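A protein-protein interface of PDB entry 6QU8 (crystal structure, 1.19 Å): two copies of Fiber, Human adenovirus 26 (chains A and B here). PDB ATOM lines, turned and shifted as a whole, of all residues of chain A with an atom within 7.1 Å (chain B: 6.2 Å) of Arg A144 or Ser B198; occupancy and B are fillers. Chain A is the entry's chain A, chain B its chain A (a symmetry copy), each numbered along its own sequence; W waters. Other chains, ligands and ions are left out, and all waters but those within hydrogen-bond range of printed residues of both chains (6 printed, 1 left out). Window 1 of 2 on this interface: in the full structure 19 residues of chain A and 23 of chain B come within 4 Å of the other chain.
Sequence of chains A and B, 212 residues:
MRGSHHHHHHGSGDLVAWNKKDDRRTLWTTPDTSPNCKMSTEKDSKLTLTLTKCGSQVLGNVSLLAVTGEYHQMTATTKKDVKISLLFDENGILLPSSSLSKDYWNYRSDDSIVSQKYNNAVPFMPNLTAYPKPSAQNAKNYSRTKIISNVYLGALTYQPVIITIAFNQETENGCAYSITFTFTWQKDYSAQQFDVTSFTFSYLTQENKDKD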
ATOM      1  N   ASN A 127       9.358 -25.713  21.059  1.00  0.00           N
ATOM      2  CA  ASN A 127      10.187 -25.616  19.837  1.00  0.00           C
ATOM      3  C   ASN A 127      11.047 -26.867  19.665  1.00  0.00           C
ATOM      4  O   ASN A 127      11.791 -27.209  20.591  1.00  0.00           O
ATOM      5  CB  ASN A 127      11.033 -24.346  19.963  1.00  0.00           C
ATOM      6  CG  ASN A 127      11.802 -24.046  18.700  1.00  0.00           C
ATOM      7  OD1 ASN A 127      12.830 -24.666  18.433  1.00  0.00           O
ATOM      8  ND2 ASN A 127      11.321 -23.056  17.960  1.00  0.00           N
ATOM      9  N   LEU A 128      10.976 -27.509  18.498  1.00  0.00           N
ATOM     10  CA  LEU A 128      11.700 -28.787  18.299  1.00  0.00           C
ATOM     11  C   LEU A 128      13.194 -28.584  18.028  1.00  0.00           C
ATOM     12  O   LEU A 128      13.935 -29.562  18.095  1.00  0.00           O
ATOM     13  CB  LEU A 128      11.020 -29.551  17.164  1.00  0.00           C
ATOM     14  CG  LEU A 128       9.788 -30.350  17.625  1.00  0.00           C
ATOM     15  CD1 LEU A 128       8.932 -30.783  16.430  1.00  0.00           C
ATOM     16  CD2 LEU A 128      10.183 -31.572  18.454  1.00  0.00           C
ATOM     17  N   THR A 129      13.619 -27.381  17.696  1.00  0.00           N
ATOM     18  CA  THR A 129      15.062 -27.082  17.548  1.00  0.00           C
ATOM     19  C   THR A 129      15.673 -26.842  18.936  1.00  0.00           C
ATOM     20  O   THR A 129      16.733 -27.417  19.270  1.00  0.00           O
ATOM     21  CB  THR A 129      15.324 -25.915  16.593  1.00  0.00           C
ATOM     22  OG1 THR A 129      14.771 -26.279  15.329  1.00  0.00           O
ATOM     23  CG2 THR A 129      16.798 -25.654  16.391  1.00  0.00           C
ATOM     24  N   ALA A 130      14.991 -26.069  19.763  1.00  0.00           N
ATOM     25  CA  ALA A 130      15.445 -25.827  21.145  1.00  0.00           C
ATOM     26  C   ALA A 130      15.387 -27.135  21.924  1.00  0.00           C
ATOM     27  O   ALA A 130      16.292 -27.423  22.732  1.00  0.00           O
ATOM     28  CB  ALA A 130      14.578 -24.786  21.804  1.00  0.00           C
ATOM     29  N   TYR A 131      14.323 -27.897  21.706  1.00  0.00           N
ATOM     30  CA  TYR A 131      14.010 -29.068  22.534  1.00  0.00           C
ATOM     31  C   TYR A 131      13.775 -30.252  21.616  1.00  0.00           C
ATOM     32  O   TYR A 131      12.639 -30.651  21.360  1.00  0.00           O
ATOM     33  CB  TYR A 131      12.812 -28.794  23.426  1.00  0.00           C
ATOM     34  CG  TYR A 131      12.778 -27.437  24.078  1.00  0.00           C
ATOM     35  CD1 TYR A 131      13.766 -27.000  24.945  1.00  0.00           C
ATOM     36  CD2 TYR A 131      11.735 -26.574  23.806  1.00  0.00           C
ATOM     37  CE1 TYR A 131      13.706 -25.741  25.524  1.00  0.00           C
ATOM     38  CE2 TYR A 131      11.654 -25.330  24.395  1.00  0.00           C
ATOM     39  CZ  TYR A 131      12.648 -24.896  25.246  1.00  0.00           C
ATOM     40  OH  TYR A 131      12.547 -23.657  25.811  1.00  0.00           O
ATOM     41  N   PRO A 132      14.850 -30.818  21.036  1.00  0.00           N
ATOM     42  CA  PRO A 132      14.695 -31.912  20.079  1.00  0.00           C
ATOM     43  C   PRO A 132      14.288 -33.206  20.789  1.00  0.00           C
ATOM     44  O   PRO A 132      14.630 -33.453  21.940  1.00  0.00           O
ATOM     45  CB  PRO A 132      16.079 -32.034  19.458  1.00  0.00           C
ATOM     46  CG  PRO A 132      17.022 -31.471  20.464  1.00  0.00           C
ATOM     47  CD  PRO A 132      16.257 -30.439  21.229  1.00  0.00           C
ATOM     48  N   ASN A 141      20.438 -36.053  26.214  1.00  0.00           N
ATOM     49  CA  ASN A 141      20.041 -34.859  25.425  1.00  0.00           C
ATOM     50  C   ASN A 141      20.556 -33.580  26.117  1.00  0.00           C
ATOM     51  O   ASN A 141      21.128 -33.605  27.204  1.00  0.00           O
ATOM     52  CB  ASN A 141      18.513 -34.801  25.206  1.00  0.00           C
ATOM     53  CG  ASN A 141      18.036 -34.094  23.940  1.00  0.00           C
ATOM     54  OD1 ASN A 141      18.786 -33.349  23.299  1.00  0.00           O
ATOM     55  ND2 ASN A 141      16.797 -34.364  23.525  1.00  0.00           N
ATOM     56  N   TYR A 142      20.307 -32.478  25.470  1.00  0.00           N
ATOM     57  CA  TYR A 142      20.604 -31.137  25.977  1.00  0.00           C
ATOM     58  C   TYR A 142      19.887 -30.907  27.316  1.00  0.00           C
ATOM     59  O   TYR A 142      18.649 -31.105  27.413  1.00  0.00           O
ATOM     60  CB  TYR A 142      20.185 -30.143  24.893  1.00  0.00           C
ATOM     61  CG  TYR A 142      20.976 -30.306  23.619  1.00  0.00           C
ATOM     62  CD1 TYR A 142      22.355 -30.197  23.654  1.00  0.00           C
ATOM     63  CD2 TYR A 142      20.364 -30.618  22.414  1.00  0.00           C
ATOM     64  CE1 TYR A 142      23.116 -30.358  22.508  1.00  0.00           C
ATOM     65  CE2 TYR A 142      21.111 -30.781  21.258  1.00  0.00           C
ATOM     66  CZ  TYR A 142      22.484 -30.655  21.321  1.00  0.00           C
ATOM     67  OH  TYR A 142      23.227 -30.812  20.207  1.00  0.00           O
ATOM     68  N   SER A 143      20.595 -30.402  28.319  1.00  0.00           N
ATOM     69  CA  SER A 143      19.956 -30.109  29.618  1.00  0.00           C
ATOM     70  C   SER A 143      18.918 -28.984  29.507  1.00  0.00           C
ATOM     71  O   SER A 143      18.029 -28.926  30.354  1.00  0.00           O
ATOM     72  CB  SER A 143      20.972 -29.773  30.675  1.00  0.00           C
ATOM     73  OG  SER A 143      21.888 -30.836  30.856  1.00  0.00           O
ATOM     74  N   ARG A 144      18.997 -28.157  28.475  1.00  0.00           N
ATOM     75  CA  ARG A 144      18.054 -27.046  28.314  1.00  0.00           C
ATOM     76  C   ARG A 144      16.639 -27.565  28.056  1.00  0.00           C
ATOM     77  O   ARG A 144      15.695 -26.775  28.179  1.00  0.00           O
ATOM     78  CB  ARG A 144      18.492 -26.091  27.208  1.00  0.00           C
ATOM     79  CG  ARG A 144      18.348 -26.648  25.802  1.00  0.00           C
ATOM     80  CD  ARG A 144      18.854 -25.624  24.764  1.00  0.00           C
ATOM     81  NE  ARG A 144      18.648 -26.160  23.433  1.00  0.00           N
ATOM     82  CZ  ARG A 144      19.280 -25.837  22.340  1.00  0.00           C
ATOM     83  NH1 ARG A 144      19.009 -26.497  21.216  1.00  0.00           N
ATOM     84  NH2 ARG A 144      20.097 -24.794  22.322  1.00  0.00           N
ATOM     85  N   THR A 145      16.478 -28.828  27.719  1.00  0.00           N
ATOM     86  CA  THR A 145      15.143 -29.439  27.549  1.00  0.00           C
ATOM     87  C   THR A 145      14.389 -29.595  28.862  1.00  0.00           C
ATOM     88  O   THR A 145      13.241 -29.991  28.809  1.00  0.00           O
ATOM     89  CB  THR A 145      15.260 -30.784  26.823  1.00  0.00           C
ATOM     90  OG1 THR A 145      15.972 -31.708  27.642  1.00  0.00           O
ATOM     91  CG2 THR A 145      15.888 -30.671  25.450  1.00  0.00           C
ATOM     92  N   LYS A 146      15.042 -29.327  29.996  1.00  0.00           N
ATOM     93  CA  LYS A 146      14.393 -29.425  31.301  1.00  0.00           C
ATOM     94  C   LYS A 146      14.500 -28.115  32.059  1.00  0.00           C
ATOM     95  O   LYS A 146      15.440 -27.333  31.892  1.00  0.00           O
ATOM     96  CB  LYS A 146      14.984 -30.570  32.102  1.00  0.00           C
ATOM     97  CG  LYS A 146      14.619 -31.937  31.540  1.00  0.00           C
ATOM     98  CD  LYS A 146      15.202 -33.077  32.260  1.00  0.00           C
ATOM     99  CE  LYS A 146      14.762 -34.408  31.702  1.00  0.00           C
ATOM    100  NZ  LYS A 146      15.392 -35.543  32.414  1.00  0.00           N
ATOM    101  N   ILE A 147      13.571 -27.956  32.971  1.00  0.00           N
ATOM    102  CA  ILE A 147      13.552 -26.967  34.060  1.00  0.00           C
ATOM    103  C   ILE A 147      13.466 -27.772  35.355  1.00  0.00           C
ATOM    104  O   ILE A 147      12.589 -28.637  35.458  1.00  0.00           O
ATOM    105  CB  ILE A 147      12.370 -26.016  33.954  1.00  0.00           C
ATOM    106  CG1 ILE A 147      12.353 -25.280  32.620  1.00  0.00           C
ATOM    107  CG2 ILE A 147      12.334 -25.070  35.140  1.00  0.00           C
ATOM    108  CD1 ILE A 147      11.007 -24.633  32.347  1.00  0.00           C
ATOM    109  N   ILE A 148      14.330 -27.476  36.318  1.00  0.00           N
ATOM    110  CA  ILE A 148      14.288 -28.169  37.622  1.00  0.00           C
ATOM    111  C   ILE A 148      14.248 -27.106  38.711  1.00  0.00           C
ATOM    112  O   ILE A 148      15.128 -26.230  38.750  1.00  0.00           O
ATOM    113  CB  ILE A 148      15.489 -29.111  37.803  1.00  0.00           C
ATOM    114  CG1 ILE A 148      15.392 -30.274  36.826  1.00  0.00           C
ATOM    115  CG2 ILE A 148      15.547 -29.614  39.233  1.00  0.00           C
ATOM    116  CD1 ILE A 148      16.590 -31.165  36.772  1.00  0.00           C
ATOM    117  N   ILE A 165      10.324 -30.149  34.729  1.00  0.00           N
ATOM    118  CA  ILE A 165       9.511 -29.954  33.512  1.00  0.00           C
ATOM    119  C   ILE A 165      10.383 -30.309  32.334  1.00  0.00           C
ATOM    120  O   ILE A 165      11.505 -29.814  32.258  1.00  0.00           O
ATOM    121  CB  ILE A 165       8.948 -28.544  33.408  1.00  0.00           C
ATOM    122  CG1 ILE A 165       8.280 -28.110  34.704  1.00  0.00           C
ATOM    123  CG2 ILE A 165       8.013 -28.448  32.227  1.00  0.00           C
ATOM    124  CD1 ILE A 165       7.691 -26.738  34.680  1.00  0.00           C
ATOM    125  N   PHE A 167      10.599 -30.912  27.993  1.00  0.00           N
ATOM    126  CA  PHE A 167       9.989 -30.554  26.709  1.00  0.00           C
ATOM    127  C   PHE A 167      10.436 -31.522  25.619  1.00  0.00           C
ATOM    128  O   PHE A 167      11.641 -31.651  25.384  1.00  0.00           O
ATOM    129  CB  PHE A 167      10.366 -29.122  26.336  1.00  0.00           C
ATOM    130  CG  PHE A 167       9.918 -28.143  27.387  1.00  0.00           C
ATOM    131  CD1 PHE A 167       8.575 -27.861  27.567  1.00  0.00           C
ATOM    132  CD2 PHE A 167      10.849 -27.517  28.195  1.00  0.00           C
ATOM    133  CE1 PHE A 167       8.167 -27.000  28.563  1.00  0.00           C
ATOM    134  CE2 PHE A 167      10.437 -26.656  29.212  1.00  0.00           C
ATOM    135  CZ  PHE A 167       9.087 -26.404  29.388  1.00  0.00           C
ATOM    136  N   SER A 202       8.663 -20.748  31.595  1.00  0.00           N
ATOM    137  CA  SER A 202       8.458 -20.381  30.189  1.00  0.00           C
ATOM    138  C   SER A 202       9.212 -21.364  29.315  1.00  0.00           C
ATOM    139  O   SER A 202      10.116 -22.076  29.777  1.00  0.00           O
ATOM    140  CB  SER A 202       8.850 -18.972  29.857  1.00  0.00           C
ATOM    141  OG  SER A 202      10.258 -18.805  29.825  1.00  0.00           O
ATOM    142  N   LEU A 204      10.343 -21.844  24.803  1.00  0.00           N
ATOM    143  CA  LEU A 204      10.362 -21.393  23.401  1.00  0.00           C
ATOM    144  C   LEU A 204       9.323 -22.186  22.614  1.00  0.00           C
ATOM    145  O   LEU A 204       9.278 -23.424  22.755  1.00  0.00           O
ATOM    146  CB  LEU A 204      11.758 -21.622  22.818  1.00  0.00           C
ATOM    147  CG  LEU A 204      12.808 -20.553  23.149  1.00  0.00           C
ATOM    148  CD1 LEU A 204      12.918 -20.217  24.624  1.00  0.00           C
ATOM    149  CD2 LEU A 204      14.171 -20.972  22.618  1.00  0.00           C
ATOM    150  N   THR B  30      18.857 -17.681  18.698  1.00  0.00           N
ATOM    151  CA  THR B  30      18.314 -18.851  17.961  1.00  0.00           C
ATOM    152  C   THR B  30      18.445 -20.068  18.865  1.00  0.00           C
ATOM    153  O   THR B  30      19.291 -20.098  19.790  1.00  0.00           O
ATOM    154  CB  THR B  30      19.008 -19.197  16.634  1.00  0.00           C
ATOM    155  OG1 THR B  30      20.293 -19.787  16.859  1.00  0.00           O
ATOM    156  CG2 THR B  30      19.157 -18.005  15.712  1.00  0.00           C
ATOM    157  N   PRO B  31      17.586 -21.079  18.625  1.00  0.00           N
ATOM    158  CA  PRO B  31      17.604 -22.282  19.440  1.00  0.00           C
ATOM    159  C   PRO B  31      18.506 -23.418  18.956  1.00  0.00           C
ATOM    160  O   PRO B  31      18.326 -24.488  19.403  1.00  0.00           O
ATOM    161  CB  PRO B  31      16.150 -22.721  19.305  1.00  0.00           C
ATOM    162  CG  PRO B  31      15.764 -22.369  17.906  1.00  0.00           C
ATOM    163  CD  PRO B  31      16.512 -21.084  17.616  1.00  0.00           C
ATOM    164  N   ASP B  32      19.425 -23.167  18.033  1.00  0.00           N
ATOM    165  CA  ASP B  32      20.303 -24.228  17.484  1.00  0.00           C
ATOM    166  C   ASP B  32      21.428 -24.483  18.501  1.00  0.00           C
ATOM    167  O   ASP B  32      21.309 -24.005  19.670  1.00  0.00           O
ATOM    168  CB  ASP B  32      20.775 -23.853  16.076  1.00  0.00           C
ATOM    169  CG  ASP B  32      21.805 -22.747  16.044  1.00  0.00           C
ATOM    170  OD1 ASP B  32      22.339 -22.398  17.129  1.00  0.00           O
ATOM    171  OD2 ASP B  32      22.084 -22.265  14.943  1.00  0.00           O
ATOM    172  N   THR B  33      22.444 -25.262  18.113  1.00  0.00           N
ATOM    173  CA  THR B  33      23.566 -25.665  19.006  1.00  0.00           C
ATOM    174  C   THR B  33      24.919 -25.153  18.479  1.00  0.00           C
ATOM    175  O   THR B  33      25.973 -25.590  19.005  1.00  0.00           O
ATOM    176  CB  THR B  33      23.512 -27.180  19.246  1.00  0.00           C
ATOM    177  OG1 THR B  33      23.600 -27.859  17.990  1.00  0.00           O
ATOM    178  CG2 THR B  33      22.247 -27.579  19.980  1.00  0.00           C
ATOM    179  N   LYS B  46      27.621 -22.736  23.770  1.00  0.00           N
ATOM    180  CA  LYS B  46      26.355 -22.246  23.197  1.00  0.00           C
ATOM    181  C   LYS B  46      25.577 -21.637  24.354  1.00  0.00           C
ATOM    182  O   LYS B  46      25.127 -22.373  25.255  1.00  0.00           O
ATOM    183  CB  LYS B  46      25.531 -23.343  22.496  1.00  0.00           C
ATOM    184  CG  LYS B  46      24.066 -22.961  22.192  1.00  0.00           C
ATOM    185  CD  LYS B  46      23.872 -22.023  20.980  1.00  0.00           C
ATOM    186  CE  LYS B  46      22.476 -21.420  20.904  1.00  0.00           C
ATOM    187  NZ  LYS B  46      22.114 -21.021  19.520  1.00  0.00           N
ATOM    188  N   THR B  48      22.053 -20.222  25.046  1.00  0.00           N
ATOM    189  CA  THR B  48      20.703 -20.148  24.473  1.00  0.00           C
ATOM    190  C   THR B  48      19.962 -19.073  25.274  1.00  0.00           C
ATOM    191  O   THR B  48      19.768 -19.241  26.470  1.00  0.00           O
ATOM    192  CB  THR B  48      19.965 -21.480  24.522  1.00  0.00           C
ATOM    193  OG1 THR B  48      20.731 -22.500  23.886  1.00  0.00           O
ATOM    194  CG2 THR B  48      18.626 -21.381  23.829  1.00  0.00           C
ATOM    195  N   ASN B  61      14.658 -16.263  29.020  1.00  0.00           N
ATOM    196  CA  ASN B  61      14.875 -17.705  29.154  1.00  0.00           C
ATOM    197  C   ASN B  61      16.317 -17.974  28.755  1.00  0.00           C
ATOM    198  O   ASN B  61      16.702 -17.567  27.659  1.00  0.00           O
ATOM    199  CB  ASN B  61      13.856 -18.441  28.306  1.00  0.00           C
ATOM    200  CG  ASN B  61      13.947 -19.924  28.374  1.00  0.00           C
ATOM    201  OD1 ASN B  61      14.823 -20.497  27.761  1.00  0.00           O
ATOM    202  ND2 ASN B  61      12.995 -20.542  29.021  1.00  0.00           N
ATOM    203  N   VAL B  62      17.072 -18.612  29.634  1.00  0.00           N
ATOM    204  CA  VAL B  62      18.530 -18.779  29.388  1.00  0.00           C
ATOM    205  C   VAL B  62      18.986 -20.192  29.759  1.00  0.00           C
ATOM    206  O   VAL B  62      18.520 -20.780  30.756  1.00  0.00           O
ATOM    207  CB  VAL B  62      19.330 -17.718  30.166  1.00  0.00           C
ATOM    208  CG1 VAL B  62      19.217 -17.863  31.668  1.00  0.00           C
ATOM    209  CG2 VAL B  62      20.794 -17.691  29.723  1.00  0.00           C
ATOM    210  N   SER B  63      19.966 -20.680  29.007  1.00  0.00           N
ATOM    211  CA  SER B  63      20.730 -21.903  29.314  1.00  0.00           C
ATOM    212  C   SER B  63      22.111 -21.798  28.672  1.00  0.00           C
ATOM    213  O   SER B  63      22.295 -20.973  27.751  1.00  0.00           O
ATOM    214  CB  SER B  63      20.003 -23.138  28.841  1.00  0.00           C
ATOM    215  OG  SER B  63      19.934 -23.146  27.423  1.00  0.00           O
ATOM    216  N   LEU B  64      23.029 -22.643  29.112  1.00  0.00           N
ATOM    217  CA  LEU B  64      24.441 -22.579  28.665  1.00  0.00           C
ATOM    218  C   LEU B  64      24.983 -23.993  28.587  1.00  0.00           C
ATOM    219  O   LEU B  64      24.754 -24.793  29.503  1.00  0.00           O
ATOM    220  CB  LEU B  64      25.244 -21.705  29.637  1.00  0.00           C
ATOM    221  CG  LEU B  64      26.736 -21.539  29.341  1.00  0.00           C
ATOM    222  CD1 LEU B  64      26.989 -20.839  28.015  1.00  0.00           C
ATOM    223  CD2 LEU B  64      27.412 -20.787  30.477  1.00  0.00           C
ATOM    224  N   VAL B 151      20.137 -23.541  38.869  1.00  0.00           N
ATOM    225  CA  VAL B 151      19.880 -24.449  37.746  1.00  0.00           C
ATOM    226  C   VAL B 151      20.667 -25.736  38.021  1.00  0.00           C
ATOM    227  O   VAL B 151      21.333 -25.831  39.051  1.00  0.00           O
ATOM    228  CB  VAL B 151      20.235 -23.792  36.405  1.00  0.00           C
ATOM    229  CG1 VAL B 151      19.298 -22.626  36.138  1.00  0.00           C
ATOM    230  CG2 VAL B 151      21.694 -23.352  36.347  1.00  0.00           C
ATOM    231  N   ALA B 155      20.979 -31.607  34.034  1.00  0.00           N
ATOM    232  CA  ALA B 155      19.578 -31.823  34.423  1.00  0.00           C
ATOM    233  C   ALA B 155      19.500 -32.944  35.453  1.00  0.00           C
ATOM    234  O   ALA B 155      18.493 -33.701  35.466  1.00  0.00           O
ATOM    235  CB  ALA B 155      18.675 -32.061  33.241  1.00  0.00           C
ATOM    236  N   ASP B 195      26.623 -28.223  31.317  1.00  0.00           N
ATOM    237  CA  ASP B 195      25.353 -28.064  30.591  1.00  0.00           C
ATOM    238  C   ASP B 195      24.328 -27.895  31.701  1.00  0.00           C
ATOM    239  O   ASP B 195      24.352 -28.660  32.648  1.00  0.00           O
ATOM    240  CB  ASP B 195      25.048 -29.286  29.743  1.00  0.00           C
ATOM    241  CG  ASP B 195      23.868 -29.107  28.807  1.00  0.00           C
ATOM    242  OD1 ASP B 195      23.403 -27.957  28.643  1.00  0.00           O
ATOM    243  OD2 ASP B 195      23.428 -30.104  28.233  1.00  0.00           O
ATOM    244  N   VAL B 196      23.464 -26.898  31.590  1.00  0.00           N
ATOM    245  CA  VAL B 196      22.490 -26.632  32.652  1.00  0.00           C
ATOM    246  C   VAL B 196      21.064 -26.577  32.114  1.00  0.00           C
ATOM    247  O   VAL B 196      20.806 -26.289  30.953  1.00  0.00           O
ATOM    248  CB  VAL B 196      22.833 -25.354  33.448  1.00  0.00           C
ATOM    249  CG1 VAL B 196      24.090 -25.565  34.256  1.00  0.00           C
ATOM    250  CG2 VAL B 196      22.949 -24.132  32.566  1.00  0.00           C
ATOM    251  N   THR B 197      20.137 -26.825  33.026  1.00  0.00           N
ATOM    252  CA  THR B 197      18.710 -26.621  32.771  1.00  0.00           C
ATOM    253  C   THR B 197      18.417 -25.161  32.452  1.00  0.00           C
ATOM    254  O   THR B 197      19.200 -24.270  32.718  1.00  0.00           O
ATOM    255  CB  THR B 197      17.913 -27.119  33.968  1.00  0.00           C
ATOM    256  OG1 THR B 197      18.363 -26.487  35.169  1.00  0.00           O
ATOM    257  CG2 THR B 197      17.986 -28.622  34.086  1.00  0.00           C
ATOM    258  N   SER B 198      17.253 -24.972  31.845  1.00  0.00           N
ATOM    259  CA  SER B 198      16.774 -23.633  31.456  1.00  0.00           C
ATOM    260  C   SER B 198      16.237 -22.873  32.664  1.00  0.00           C
ATOM    261  O   SER B 198      15.629 -23.451  33.568  1.00  0.00           O
ATOM    262  CB  SER B 198      15.713 -23.741  30.376  1.00  0.00           C
ATOM    263  OG  SER B 198      16.223 -24.245  29.161  1.00  0.00           O
ATOM    264  N   PHE B 199      16.399 -21.556  32.602  1.00  0.00           N
ATOM    265  CA  PHE B 199      15.965 -20.655  33.671  1.00  0.00           C
ATOM    266  C   PHE B 199      15.149 -19.511  33.091  1.00  0.00           C
ATOM    267  O   PHE B 199      15.612 -18.820  32.178  1.00  0.00           O
ATOM    268  CB  PHE B 199      17.172 -20.125  34.447  1.00  0.00           C
ATOM    269  CG  PHE B 199      16.780 -19.358  35.677  1.00  0.00           C
ATOM    270  CD1 PHE B 199      16.267 -20.002  36.780  1.00  0.00           C
ATOM    271  CD2 PHE B 199      16.905 -17.979  35.736  1.00  0.00           C
ATOM    272  CE1 PHE B 199      15.888 -19.292  37.898  1.00  0.00           C
ATOM    273  CE2 PHE B 199      16.543 -17.260  36.853  1.00  0.00           C
ATOM    274  CZ  PHE B 199      16.011 -17.922  37.914  1.00  0.00           C
ATOM    275  N   THR B 200      13.983 -19.296  33.691  1.00  0.00           N
ATOM    276  CA  THR B 200      13.018 -18.252  33.321  1.00  0.00           C
ATOM    277  C   THR B 200      13.216 -17.072  34.272  1.00  0.00           C
ATOM    278  O   THR B 200      13.448 -17.279  35.466  1.00  0.00           O
ATOM    279  CB  THR B 200      11.587 -18.793  33.267  1.00  0.00           C
ATOM    280  OG1 THR B 200      11.554 -19.697  32.135  1.00  0.00           O
ATOM    281  CG2 THR B 200      10.560 -17.713  32.965  1.00  0.00           C
HETATM  282  O   HOH W   1      14.893 -23.016  26.997  1.00  0.00           O
HETATM  283  O   HOH W   2      16.121 -25.071  35.653  1.00  0.00           O
HETATM  284  O   HOH W   3      21.389 -27.955  26.671  1.00  0.00           O
HETATM  285  O   HOH W   4      12.525 -23.305  29.499  1.00  0.00           O
HETATM  286  O   HOH W   5      18.290 -35.516  33.037  1.00  0.00           O
HETATM  287  O   HOH W   6      13.398 -25.883  29.145  1.00  0.00           O
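The backbone carbonyl oxygen of Asp B32 is in hydrogen-bond range of the guanidinium group of Arg A144 (3.0 Å). The side-chain amide nitrogen (ND2) of Asn B61 sits at hydrogen-bond distance from the side-chain hydroxyl (OG) of Ser A202, 3.3 Å away. The backbone carbonyl oxygen of Pro B31 lies within hydrogen-bond range of the guanidinium group of Arg A144 (2.8 Å). NH2 of Arg A144 lies within hydrogen-bond range of OG1 of Thr B48. The backbone NH of Ala B155 lies within hydrogen-bond range of the side-chain hydroxyl of Ser A143 (3.4 Å). OG of Ser B198 sits at hydrogen-bond distance from O of Arg A144 (2.8 Å). The backbone carbonyl oxygen (O) of Pro B31 sits close to the backbone carbonyl oxygen (O) of Thr A129, 3.3 Å away. The side-chain hydroxyl (OG) of Ser A202 sits at hydrogen-bond distance from the side-chain hydroxyl (OG1) of Thr B200 (2.8 Å). The backbone NH (N) of Ser B198 sits at hydrogen-bond distance from the backbone carbonyl oxygen (O) of Lys A146 (3.0 Å). N of Ser A143 sits at hydrogen-bond distance from OD2 of Asp B195, 2.8 Å away.
The backbone carbonyl oxygen of Ile A147 sits at hydrogen-bond distance from the backbone NH of Ile A165 (2.8 Å). O of Ser B63 sits at hydrogen-bond distance from N of Thr B48, 2.8 Å away. O of Leu A204 lies within hydrogen-bond range of N of Asn A127, 2.8 Å away. OH of Tyr A131 lies within hydrogen-bond range of N of Leu A204 (3.0 Å). OD1 of Asp B32 sits at hydrogen-bond distance from OG1 of Thr B30 (3.3 Å). The guanidinium group of Arg A144 lies within hydrogen-bond range of the backbone carbonyl oxygen of Thr A129 (3.1 Å).
Thr A129 touches Asp B32 (CG2 to CA, 3.9 Å). Ala A130 touches Pro B31. CA of Thr B197 touches O of Ser A143, 3.4 Å away. Arg A144 touches Thr B33. CB of Arg A144 touches OG of Ser B63 (3.3 Å). N of Arg A144 touches O of Val B196 (3.6 Å). O of Lys A146 touches CB of Thr B197 (3.2 Å). Ile A148 touches Ala B155. CD1 of Ile A148 touches CG2 of Thr B197, 3.95 Å away. Leu A204 touches Asn B61 (CD1 to OD1, 3.7 Å).
Printed residues of chain B within 4 Å of Arg A144: Pro B31 (2.8 Å), Asp B32 (3.0 Å), Thr B33 (3.6 Å), Thr B48 (2.8 Å), Ser B63 (3.3 Å), Val B196 (3.6 Å) and Ser B198 (2.8 Å). Of chain A, only Arg A144 (2.8 Å), Lys A146 (3.0 Å) and Ile A147 (3.9 Å) come within 4 Å of Ser B198. Of the printed residues of chain B, Tyr A142 touches Thr B33 (3.4 Å) and Asp B195 (3.7 Å). Of the printed residues of chain A, Asn B61 touches Ser A202 and Leu A204. Tyr A131 touches none of the printed residues of chain B. Ile A165 touches none of the printed residues of chain B. The nearest printed residue of chain A that does not touch Ser B63 is Ser A143 (6.0 Å).
Printed residues of chain A that touch a printed residue of chain B: Asn A127, Thr A129, Ala A130, Tyr A142, Ser A143, Arg A144, Lys A146, Ile A147, Ile A148, Ser A202 and Leu A204. Among the printed residues, 26 pairs touch across the chains.
No position is printed for both chains. Of the 26 pairs that touch across the chains among the printed residues, none has its exchanged pair printed and touching as well.
Water W1 lies within hydrogen-bond range of OD1 of Asn B61 (2.6 Å), OH of Tyr A131 (2.7 Å) and OG of Ser B198 (2.8 Å). Water W6 lies within hydrogen-bond range of the backbone carbonyl oxygen (O) of Arg A144 and the side-chain hydroxyl (OG) of Ser B198. Water W2 lies within hydrogen-bond range of the backbone carbonyl oxygen (O) of Ser B198 (2.7 Å), the side-chain hydroxyl (OG1) of Thr B197 (2.7 Å) and the backbone NH (N) of Ile A148 (3.1 Å). Water W4 bridges O of Ser A202 (2.7 Å) and ND2 of Asn B61 (2.8 Å). Water W3 lies within hydrogen-bond range of OD1 of Asp B195, N of Arg A144 and N of Ser A143. Water W5 lies within hydrogen-bond range of NZ of Lys A146 (3.0 Å) and O of Ala B155 (3.0 Å).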
